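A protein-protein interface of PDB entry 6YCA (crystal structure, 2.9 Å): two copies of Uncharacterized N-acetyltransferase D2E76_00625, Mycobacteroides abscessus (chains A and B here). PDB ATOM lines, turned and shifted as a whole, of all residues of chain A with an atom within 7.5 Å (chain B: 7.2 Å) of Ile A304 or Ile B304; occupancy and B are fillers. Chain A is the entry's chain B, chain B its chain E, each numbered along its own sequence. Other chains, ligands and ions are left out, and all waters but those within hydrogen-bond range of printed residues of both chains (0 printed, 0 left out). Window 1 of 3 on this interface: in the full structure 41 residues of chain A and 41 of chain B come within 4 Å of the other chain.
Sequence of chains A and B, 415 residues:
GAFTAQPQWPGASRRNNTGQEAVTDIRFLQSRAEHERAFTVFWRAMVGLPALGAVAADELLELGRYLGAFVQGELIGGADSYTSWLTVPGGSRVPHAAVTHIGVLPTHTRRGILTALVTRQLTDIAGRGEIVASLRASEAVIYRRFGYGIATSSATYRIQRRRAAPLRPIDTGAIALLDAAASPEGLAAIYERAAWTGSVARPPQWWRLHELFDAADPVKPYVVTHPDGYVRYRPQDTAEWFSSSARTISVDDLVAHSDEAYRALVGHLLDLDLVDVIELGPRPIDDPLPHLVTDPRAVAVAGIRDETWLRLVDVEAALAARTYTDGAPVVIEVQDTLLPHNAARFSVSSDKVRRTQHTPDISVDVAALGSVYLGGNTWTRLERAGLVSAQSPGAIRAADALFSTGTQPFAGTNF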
ATOM      1  N   SER A 153      13.737 -27.543  38.785  1.00  0.00           N
ATOM      2  CA  SER A 153      13.314 -27.077  37.474  1.00  0.00           C
ATOM      3  C   SER A 153      13.889 -28.003  36.410  1.00  0.00           C
ATOM      4  O   SER A 153      14.833 -28.758  36.660  1.00  0.00           O
ATOM      5  CB  SER A 153      13.744 -25.627  37.205  1.00  0.00           C
ATOM      6  OG  SER A 153      13.148 -24.733  38.129  1.00  0.00           O
ATOM      7  N   SER A 154      13.287 -27.958  35.227  1.00  0.00           N
ATOM      8  CA  SER A 154      13.699 -28.765  34.090  1.00  0.00           C
ATOM      9  C   SER A 154      13.992 -27.857  32.903  1.00  0.00           C
ATOM     10  O   SER A 154      13.458 -26.749  32.799  1.00  0.00           O
ATOM     11  CB  SER A 154      12.609 -29.777  33.715  1.00  0.00           C
ATOM     12  OG  SER A 154      11.487 -29.129  33.141  1.00  0.00           O
ATOM     13  N   ALA A 155      14.835 -28.342  31.992  1.00  0.00           N
ATOM     14  CA  ALA A 155      15.259 -27.563  30.836  1.00  0.00           C
ATOM     15  C   ALA A 155      14.997 -28.332  29.549  1.00  0.00           C
ATOM     16  O   ALA A 155      14.814 -29.553  29.551  1.00  0.00           O
ATOM     17  CB  ALA A 155      16.747 -27.195  30.909  1.00  0.00           C
ATOM     18  N   THR A 156      14.969 -27.590  28.445  1.00  0.00           N
ATOM     19  CA  THR A 156      14.798 -28.147  27.110  1.00  0.00           C
ATOM     20  C   THR A 156      15.969 -27.686  26.254  1.00  0.00           C
ATOM     21  O   THR A 156      16.199 -26.480  26.117  1.00  0.00           O
ATOM     22  CB  THR A 156      13.496 -27.643  26.494  1.00  0.00           C
ATOM     23  OG1 THR A 156      12.414 -27.894  27.396  1.00  0.00           O
ATOM     24  CG2 THR A 156      13.229 -28.349  25.172  1.00  0.00           C
ATOM     25  N   TYR A 157      16.693 -28.639  25.672  1.00  0.00           N
ATOM     26  CA  TYR A 157      17.861 -28.361  24.850  1.00  0.00           C
ATOM     27  C   TYR A 157      17.573 -28.738  23.404  1.00  0.00           C
ATOM     28  O   TYR A 157      16.941 -29.765  23.141  1.00  0.00           O
ATOM     29  CB  TYR A 157      19.067 -29.174  25.330  1.00  0.00           C
ATOM     30  CG  TYR A 157      19.462 -28.905  26.763  1.00  0.00           C
ATOM     31  CD1 TYR A 157      20.201 -27.778  27.100  1.00  0.00           C
ATOM     32  CD2 TYR A 157      19.101 -29.776  27.776  1.00  0.00           C
ATOM     33  CE1 TYR A 157      20.565 -27.527  28.407  1.00  0.00           C
ATOM     34  CE2 TYR A 157      19.459 -29.532  29.086  1.00  0.00           C
ATOM     35  CZ  TYR A 157      20.191 -28.408  29.397  1.00  0.00           C
ATOM     36  OH  TYR A 157      20.549 -28.163  30.704  1.00  0.00           O
ATOM     37  N   ARG A 283      15.155 -32.013  30.791  1.00  0.00           N
ATOM     38  CA  ARG A 283      16.474 -32.392  31.270  1.00  0.00           C
ATOM     39  C   ARG A 283      16.881 -31.494  32.427  1.00  0.00           C
ATOM     40  O   ARG A 283      16.271 -30.442  32.653  1.00  0.00           O
ATOM     41  CB  ARG A 283      17.497 -32.282  30.130  1.00  0.00           C
ATOM     42  CG  ARG A 283      17.313 -33.328  29.034  1.00  0.00           C
ATOM     43  CD  ARG A 283      17.477 -34.733  29.571  1.00  0.00           C
ATOM     44  NE  ARG A 283      18.771 -34.901  30.226  1.00  0.00           N
ATOM     45  CZ  ARG A 283      19.084 -35.923  31.016  1.00  0.00           C
ATOM     46  NH1 ARG A 283      18.192 -36.881  31.248  1.00  0.00           N
ATOM     47  NH2 ARG A 283      20.290 -35.985  31.569  1.00  0.00           N
ATOM     48  N   ILE A 285      18.652 -28.646  34.568  1.00  0.00           N
ATOM     49  CA  ILE A 285      19.084 -27.319  34.139  1.00  0.00           C
ATOM     50  C   ILE A 285      20.606 -27.192  34.087  1.00  0.00           C
ATOM     51  O   ILE A 285      21.119 -26.261  33.454  1.00  0.00           O
ATOM     52  CB  ILE A 285      18.389 -26.181  34.921  1.00  0.00           C
ATOM     53  CG1 ILE A 285      18.831 -26.164  36.385  1.00  0.00           C
ATOM     54  CG2 ILE A 285      16.879 -26.313  34.824  1.00  0.00           C
ATOM     55  CD1 ILE A 285      18.278 -24.996  37.173  1.00  0.00           C
ATOM     56  N   ARG A 297      27.863 -23.769  21.598  1.00  0.00           N
ATOM     57  CA  ARG A 297      26.702 -23.108  21.020  1.00  0.00           C
ATOM     58  C   ARG A 297      25.924 -24.006  20.070  1.00  0.00           C
ATOM     59  O   ARG A 297      24.858 -23.600  19.598  1.00  0.00           O
ATOM     60  CB  ARG A 297      27.121 -21.809  20.332  1.00  0.00           C
ATOM     61  CG  ARG A 297      27.634 -20.775  21.319  1.00  0.00           C
ATOM     62  CD  ARG A 297      28.148 -19.528  20.637  1.00  0.00           C
ATOM     63  NE  ARG A 297      28.819 -18.637  21.579  1.00  0.00           N
ATOM     64  CZ  ARG A 297      29.527 -17.572  21.218  1.00  0.00           C
ATOM     65  NH1 ARG A 297      29.656 -17.269  19.934  1.00  0.00           N
ATOM     66  NH2 ARG A 297      30.112 -16.816  22.137  1.00  0.00           N
ATOM     67  N   VAL A 299      24.619 -26.490  21.316  1.00  0.00           N
ATOM     68  CA  VAL A 299      23.617 -26.896  22.289  1.00  0.00           C
ATOM     69  C   VAL A 299      22.962 -25.619  22.784  1.00  0.00           C
ATOM     70  O   VAL A 299      23.614 -24.792  23.431  1.00  0.00           O
ATOM     71  CB  VAL A 299      24.251 -27.671  23.448  1.00  0.00           C
ATOM     72  CG1 VAL A 299      23.182 -28.150  24.410  1.00  0.00           C
ATOM     73  CG2 VAL A 299      25.088 -28.829  22.917  1.00  0.00           C
ATOM     74  N   ALA A 300      21.677 -25.453  22.488  1.00  0.00           N
ATOM     75  CA  ALA A 300      20.933 -24.258  22.853  1.00  0.00           C
ATOM     76  C   ALA A 300      19.827 -24.611  23.835  1.00  0.00           C
ATOM     77  O   ALA A 300      19.131 -25.617  23.670  1.00  0.00           O
ATOM     78  CB  ALA A 300      20.310 -23.608  21.619  1.00  0.00           C
ATOM     79  N   VAL A 301      19.668 -23.776  24.859  1.00  0.00           N
ATOM     80  CA  VAL A 301      18.586 -23.943  25.821  1.00  0.00           C
ATOM     81  C   VAL A 301      17.332 -23.317  25.223  1.00  0.00           C
ATOM     82  O   VAL A 301      17.242 -22.094  25.092  1.00  0.00           O
ATOM     83  CB  VAL A 301      18.935 -23.305  27.167  1.00  0.00           C
ATOM     84  CG1 VAL A 301      17.731 -23.352  28.100  1.00  0.00           C
ATOM     85  CG2 VAL A 301      20.139 -23.999  27.776  1.00  0.00           C
ATOM     86  N   ALA A 302      16.369 -24.154  24.847  1.00  0.00           N
ATOM     87  CA  ALA A 302      15.122 -23.697  24.250  1.00  0.00           C
ATOM     88  C   ALA A 302      14.042 -23.368  25.275  1.00  0.00           C
ATOM     89  O   ALA A 302      12.956 -22.930  24.883  1.00  0.00           O
ATOM     90  CB  ALA A 302      14.592 -24.725  23.247  1.00  0.00           C
ATOM     91  N   GLY A 303      14.303 -23.561  26.568  1.00  0.00           N
ATOM     92  CA  GLY A 303      13.299 -23.247  27.568  1.00  0.00           C
ATOM     93  C   GLY A 303      13.571 -23.801  28.952  1.00  0.00           C
ATOM     94  O   GLY A 303      14.254 -24.819  29.104  1.00  0.00           O
ATOM     95  N   ILE A 304      13.042 -23.132  29.973  1.00  0.00           N
ATOM     96  CA  ILE A 304      13.188 -23.560  31.359  1.00  0.00           C
ATOM     97  C   ILE A 304      11.841 -23.415  32.054  1.00  0.00           C
ATOM     98  O   ILE A 304      11.193 -22.367  31.950  1.00  0.00           O
ATOM     99  CB  ILE A 304      14.278 -22.760  32.100  1.00  0.00           C
ATOM    100  CG1 ILE A 304      15.667 -23.175  31.621  1.00  0.00           C
ATOM    101  CG2 ILE A 304      14.159 -22.943  33.609  1.00  0.00           C
ATOM    102  CD1 ILE A 304      16.791 -22.459  32.342  1.00  0.00           C
ATOM    103  N   ARG A 305      11.439 -24.453  32.789  1.00  0.00           N
ATOM    104  CA  ARG A 305      10.126 -24.534  33.407  1.00  0.00           C
ATOM    105  C   ARG A 305      10.276 -25.054  34.827  1.00  0.00           C
ATOM    106  O   ARG A 305      11.203 -25.811  35.132  1.00  0.00           O
ATOM    107  CB  ARG A 305       9.270 -25.550  32.648  1.00  0.00           C
ATOM    108  CG  ARG A 305       7.800 -25.601  33.043  1.00  0.00           C
ATOM    109  CD  ARG A 305       7.011 -24.467  32.419  1.00  0.00           C
ATOM    110  NE  ARG A 305       5.575 -24.695  32.522  1.00  0.00           N
ATOM    111  CZ  ARG A 305       4.656 -23.900  31.987  1.00  0.00           C
ATOM    112  NH1 ARG A 305       5.025 -22.815  31.320  1.00  0.00           N
ATOM    113  NH2 ARG A 305       3.367 -24.186  32.121  1.00  0.00           N
ATOM    114  N   ASP A 306       9.368 -24.627  35.702  1.00  0.00           N
ATOM    115  CA  ASP A 306       9.317 -25.206  37.036  1.00  0.00           C
ATOM    116  C   ASP A 306       8.917 -26.674  36.938  1.00  0.00           C
ATOM    117  O   ASP A 306       8.128 -27.072  36.074  1.00  0.00           O
ATOM    118  CB  ASP A 306       8.313 -24.462  37.915  1.00  0.00           C
ATOM    119  CG  ASP A 306       6.949 -24.346  37.269  1.00  0.00           C
ATOM    120  OD1 ASP A 306       6.846 -23.686  36.216  1.00  0.00           O
ATOM    121  OD2 ASP A 306       5.986 -24.948  37.789  1.00  0.00           O
ATOM    122  N   GLU A 307       9.466 -27.485  37.844  1.00  0.00           N
ATOM    123  CA  GLU A 307       9.219 -28.922  37.830  1.00  0.00           C
ATOM    124  C   GLU A 307       8.588 -29.410  39.125  1.00  0.00           C
ATOM    125  O   GLU A 307       7.371 -29.615  39.185  1.00  0.00           O
ATOM    126  CB  GLU A 307      10.509 -29.694  37.556  1.00  0.00           C
ATOM    127  CG  GLU A 307      10.280 -31.177  37.357  1.00  0.00           C
ATOM    128  CD  GLU A 307      11.558 -31.951  37.123  1.00  0.00           C
ATOM    129  OE1 GLU A 307      12.548 -31.696  37.843  1.00  0.00           O
ATOM    130  OE2 GLU A 307      11.557 -32.840  36.242  1.00  0.00           O
ATOM    131  N   SER B 153      27.680 -17.583  32.581  1.00  0.00           N
ATOM    132  CA  SER B 153      26.668 -17.536  31.541  1.00  0.00           C
ATOM    133  C   SER B 153      25.649 -16.461  31.889  1.00  0.00           C
ATOM    134  O   SER B 153      25.540 -16.027  33.040  1.00  0.00           O
ATOM    135  CB  SER B 153      25.974 -18.891  31.355  1.00  0.00           C
ATOM    136  OG  SER B 153      26.904 -19.881  30.953  1.00  0.00           O
ATOM    137  N   SER B 154      24.911 -16.025  30.871  1.00  0.00           N
ATOM    138  CA  SER B 154      23.904 -14.985  31.008  1.00  0.00           C
ATOM    139  C   SER B 154      22.557 -15.498  30.519  1.00  0.00           C
ATOM    140  O   SER B 154      22.476 -16.427  29.714  1.00  0.00           O
ATOM    141  CB  SER B 154      24.292 -13.740  30.204  1.00  0.00           C
ATOM    142  OG  SER B 154      24.179 -13.980  28.810  1.00  0.00           O
ATOM    143  N   ALA B 155      21.489 -14.883  31.019  1.00  0.00           N
ATOM    144  CA  ALA B 155      20.131 -15.270  30.662  1.00  0.00           C
ATOM    145  C   ALA B 155      19.350 -14.056  30.175  1.00  0.00           C
ATOM    146  O   ALA B 155      19.718 -12.905  30.428  1.00  0.00           O
ATOM    147  CB  ALA B 155      19.394 -15.913  31.845  1.00  0.00           C
ATOM    148  N   THR B 156      18.266 -14.332  29.456  1.00  0.00           N
ATOM    149  CA  THR B 156      17.341 -13.311  28.980  1.00  0.00           C
ATOM    150  C   THR B 156      15.955 -13.674  29.488  1.00  0.00           C
ATOM    151  O   THR B 156      15.448 -14.760  29.189  1.00  0.00           O
ATOM    152  CB  THR B 156      17.331 -13.269  27.454  1.00  0.00           C
ATOM    153  OG1 THR B 156      18.670 -13.113  26.976  1.00  0.00           O
ATOM    154  CG2 THR B 156      16.475 -12.114  26.960  1.00  0.00           C
ATOM    155  N   TYR B 157      15.332 -12.760  30.226  1.00  0.00           N
ATOM    156  CA  TYR B 157      14.033 -12.997  30.840  1.00  0.00           C
ATOM    157  C   TYR B 157      12.983 -12.120  30.175  1.00  0.00           C
ATOM    158  O   TYR B 157      13.237 -10.950  29.876  1.00  0.00           O
ATOM    159  CB  TYR B 157      14.076 -12.684  32.339  1.00  0.00           C
ATOM    160  CG  TYR B 157      15.083 -13.504  33.107  1.00  0.00           C
ATOM    161  CD1 TYR B 157      16.410 -13.113  33.183  1.00  0.00           C
ATOM    162  CD2 TYR B 157      14.705 -14.674  33.755  1.00  0.00           C
ATOM    163  CE1 TYR B 157      17.335 -13.861  33.883  1.00  0.00           C
ATOM    164  CE2 TYR B 157      15.621 -15.430  34.459  1.00  0.00           C
ATOM    165  CZ  TYR B 157      16.937 -15.019  34.522  1.00  0.00           C
ATOM    166  OH  TYR B 157      17.859 -15.768  35.220  1.00  0.00           O
ATOM    167  N   ILE B 285      22.004 -16.198  35.430  1.00  0.00           N
ATOM    168  CA  ILE B 285      21.167 -17.363  35.159  1.00  0.00           C
ATOM    169  C   ILE B 285      20.350 -17.766  36.379  1.00  0.00           C
ATOM    170  O   ILE B 285      19.370 -18.504  36.243  1.00  0.00           O
ATOM    171  CB  ILE B 285      21.981 -18.537  34.576  1.00  0.00           C
ATOM    172  CG1 ILE B 285      22.938 -19.106  35.626  1.00  0.00           C
ATOM    173  CG2 ILE B 285      22.748 -18.092  33.337  1.00  0.00           C
ATOM    174  CD1 ILE B 285      23.688 -20.344  35.174  1.00  0.00           C
ATOM    175  N   VAL B 299       7.453 -15.052  34.493  1.00  0.00           N
ATOM    176  CA  VAL B 299       8.850 -14.839  34.135  1.00  0.00           C
ATOM    177  C   VAL B 299       9.309 -16.049  33.337  1.00  0.00           C
ATOM    178  O   VAL B 299       9.346 -17.170  33.861  1.00  0.00           O
ATOM    179  CB  VAL B 299       9.723 -14.649  35.385  1.00  0.00           C
ATOM    180  CG1 VAL B 299      11.160 -14.402  34.989  1.00  0.00           C
ATOM    181  CG2 VAL B 299       9.204 -13.497  36.223  1.00  0.00           C
ATOM    182  N   ALA B 300       9.638 -15.833  32.067  1.00  0.00           N
ATOM    183  CA  ALA B 300      10.079 -16.893  31.173  1.00  0.00           C
ATOM    184  C   ALA B 300      11.508 -16.626  30.728  1.00  0.00           C
ATOM    185  O   ALA B 300      11.856 -15.493  30.372  1.00  0.00           O
ATOM    186  CB  ALA B 300       9.186 -16.962  29.941  1.00  0.00           C
ATOM    187  N   VAL B 301      12.330 -17.672  30.723  1.00  0.00           N
ATOM    188  CA  VAL B 301      13.698 -17.559  30.228  1.00  0.00           C
ATOM    189  C   VAL B 301      13.653 -17.667  28.707  1.00  0.00           C
ATOM    190  O   VAL B 301      13.397 -18.739  28.156  1.00  0.00           O
ATOM    191  CB  VAL B 301      14.613 -18.625  30.840  1.00  0.00           C
ATOM    192  CG1 VAL B 301      15.970 -18.593  30.173  1.00  0.00           C
ATOM    193  CG2 VAL B 301      14.762 -18.391  32.332  1.00  0.00           C
ATOM    194  N   ALA B 302      13.907 -16.553  28.028  1.00  0.00           N
ATOM    195  CA  ALA B 302      13.866 -16.481  26.574  1.00  0.00           C
ATOM    196  C   ALA B 302      15.181 -16.879  25.917  1.00  0.00           C
ATOM    197  O   ALA B 302      15.271 -16.855  24.684  1.00  0.00           O
ATOM    198  CB  ALA B 302      13.449 -15.077  26.120  1.00  0.00           C
ATOM    199  N   GLY B 303      16.203 -17.222  26.698  1.00  0.00           N
ATOM    200  CA  GLY B 303      17.469 -17.650  26.137  1.00  0.00           C
ATOM    201  C   GLY B 303      18.600 -17.672  27.142  1.00  0.00           C
ATOM    202  O   GLY B 303      18.598 -16.904  28.108  1.00  0.00           O
ATOM    203  N   ILE B 304      19.577 -18.545  26.921  1.00  0.00           N
ATOM    204  CA  ILE B 304      20.746 -18.659  27.782  1.00  0.00           C
ATOM    205  C   ILE B 304      21.974 -18.765  26.893  1.00  0.00           C
ATOM    206  O   ILE B 304      21.978 -19.511  25.911  1.00  0.00           O
ATOM    207  CB  ILE B 304      20.628 -19.841  28.770  1.00  0.00           C
ATOM    208  CG1 ILE B 304      19.625 -19.495  29.874  1.00  0.00           C
ATOM    209  CG2 ILE B 304      21.972 -20.194  29.372  1.00  0.00           C
ATOM    210  CD1 ILE B 304      19.476 -20.560  30.936  1.00  0.00           C
ATOM    211  N   ARG B 305      23.007 -17.997  27.222  1.00  0.00           N
ATOM    212  CA  ARG B 305      24.192 -17.883  26.386  1.00  0.00           C
ATOM    213  C   ARG B 305      25.443 -17.916  27.253  1.00  0.00           C
ATOM    214  O   ARG B 305      25.419 -17.522  28.424  1.00  0.00           O
ATOM    215  CB  ARG B 305      24.157 -16.567  25.610  1.00  0.00           C
ATOM    216  CG  ARG B 305      25.215 -16.406  24.534  1.00  0.00           C
ATOM    217  CD  ARG B 305      24.852 -17.164  23.276  1.00  0.00           C
ATOM    218  NE  ARG B 305      25.672 -16.741  22.147  1.00  0.00           N
ATOM    219  CZ  ARG B 305      25.503 -17.181  20.906  1.00  0.00           C
ATOM    220  NH1 ARG B 305      24.547 -18.062  20.645  1.00  0.00           N
ATOM    221  NH2 ARG B 305      26.284 -16.742  19.924  1.00  0.00           N
ATOM    222  N   ASP B 306      26.527 -18.435  26.676  1.00  0.00           N
ATOM    223  CA  ASP B 306      27.828 -18.357  27.325  1.00  0.00           C
ATOM    224  C   ASP B 306      28.273 -16.902  27.402  1.00  0.00           C
ATOM    225  O   ASP B 306      27.972 -16.093  26.523  1.00  0.00           O
ATOM    226  CB  ASP B 306      28.856 -19.164  26.543  1.00  0.00           C
ATOM    227  CG  ASP B 306      28.891 -18.790  25.077  1.00  0.00           C
ATOM    228  OD1 ASP B 306      27.855 -18.979  24.398  1.00  0.00           O
ATOM    229  OD2 ASP B 306      29.939 -18.311  24.602  1.00  0.00           O
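The guanidinium group (NH1) of Arg A297 sits close to the guanidinium group (NH2) of Arg B305.
OD2 of Asp B306 is in salt-bridge range of NH2 of Arg A297 (2.9 Å).
The backbone NH (N) of Ser B154 sits at hydrogen-bond distance from the backbone carbonyl oxygen (O) of Arg B305, 2.9 Å away.
The guanidinium group (NE) of Arg B305 is in salt-bridge range of the side-chain carboxylate (OD1) of Asp B306.
Among the printed residues, pairs that only touch across the chains: Ile A304 with Ile B304.
Ile A304 touches one residue of chain B.
Printed residues of chain A within 4 Å of Ile B304: Ile A304.
Of the printed residues of chain A, Arg B305 touches Arg A297.
Of the printed residues of chain B, Arg A297 touches Arg B305 and Asp B306.
Of the printed residues of chain A, Asp B306 touches Arg A297.
Glu A307 touches none of the printed residues of chain B.
Tyr A157 touches none of the printed residues of chain B.
The nearest residue of chain B that does not touch Ile A304 is Val B301 (4.3 Å).
The nearest printed residue of chain A that does not touch Arg B305 is Val A301 (6.7 Å).
Printed residues of chain B that touch a printed residue of chain A: Ile B304, Arg B305 and Asp B306.
Hydrophobic or aromatic side chains of chain B within 4 Å of the printed part of chain A: Ile B304.
Ile A304 touches its own counterpart, Ile B304.
Positions printed for both chains: 153, 154, 155, 156, 157, 285, 299, 300, 301, 302, 303, 304, 305 and 306.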
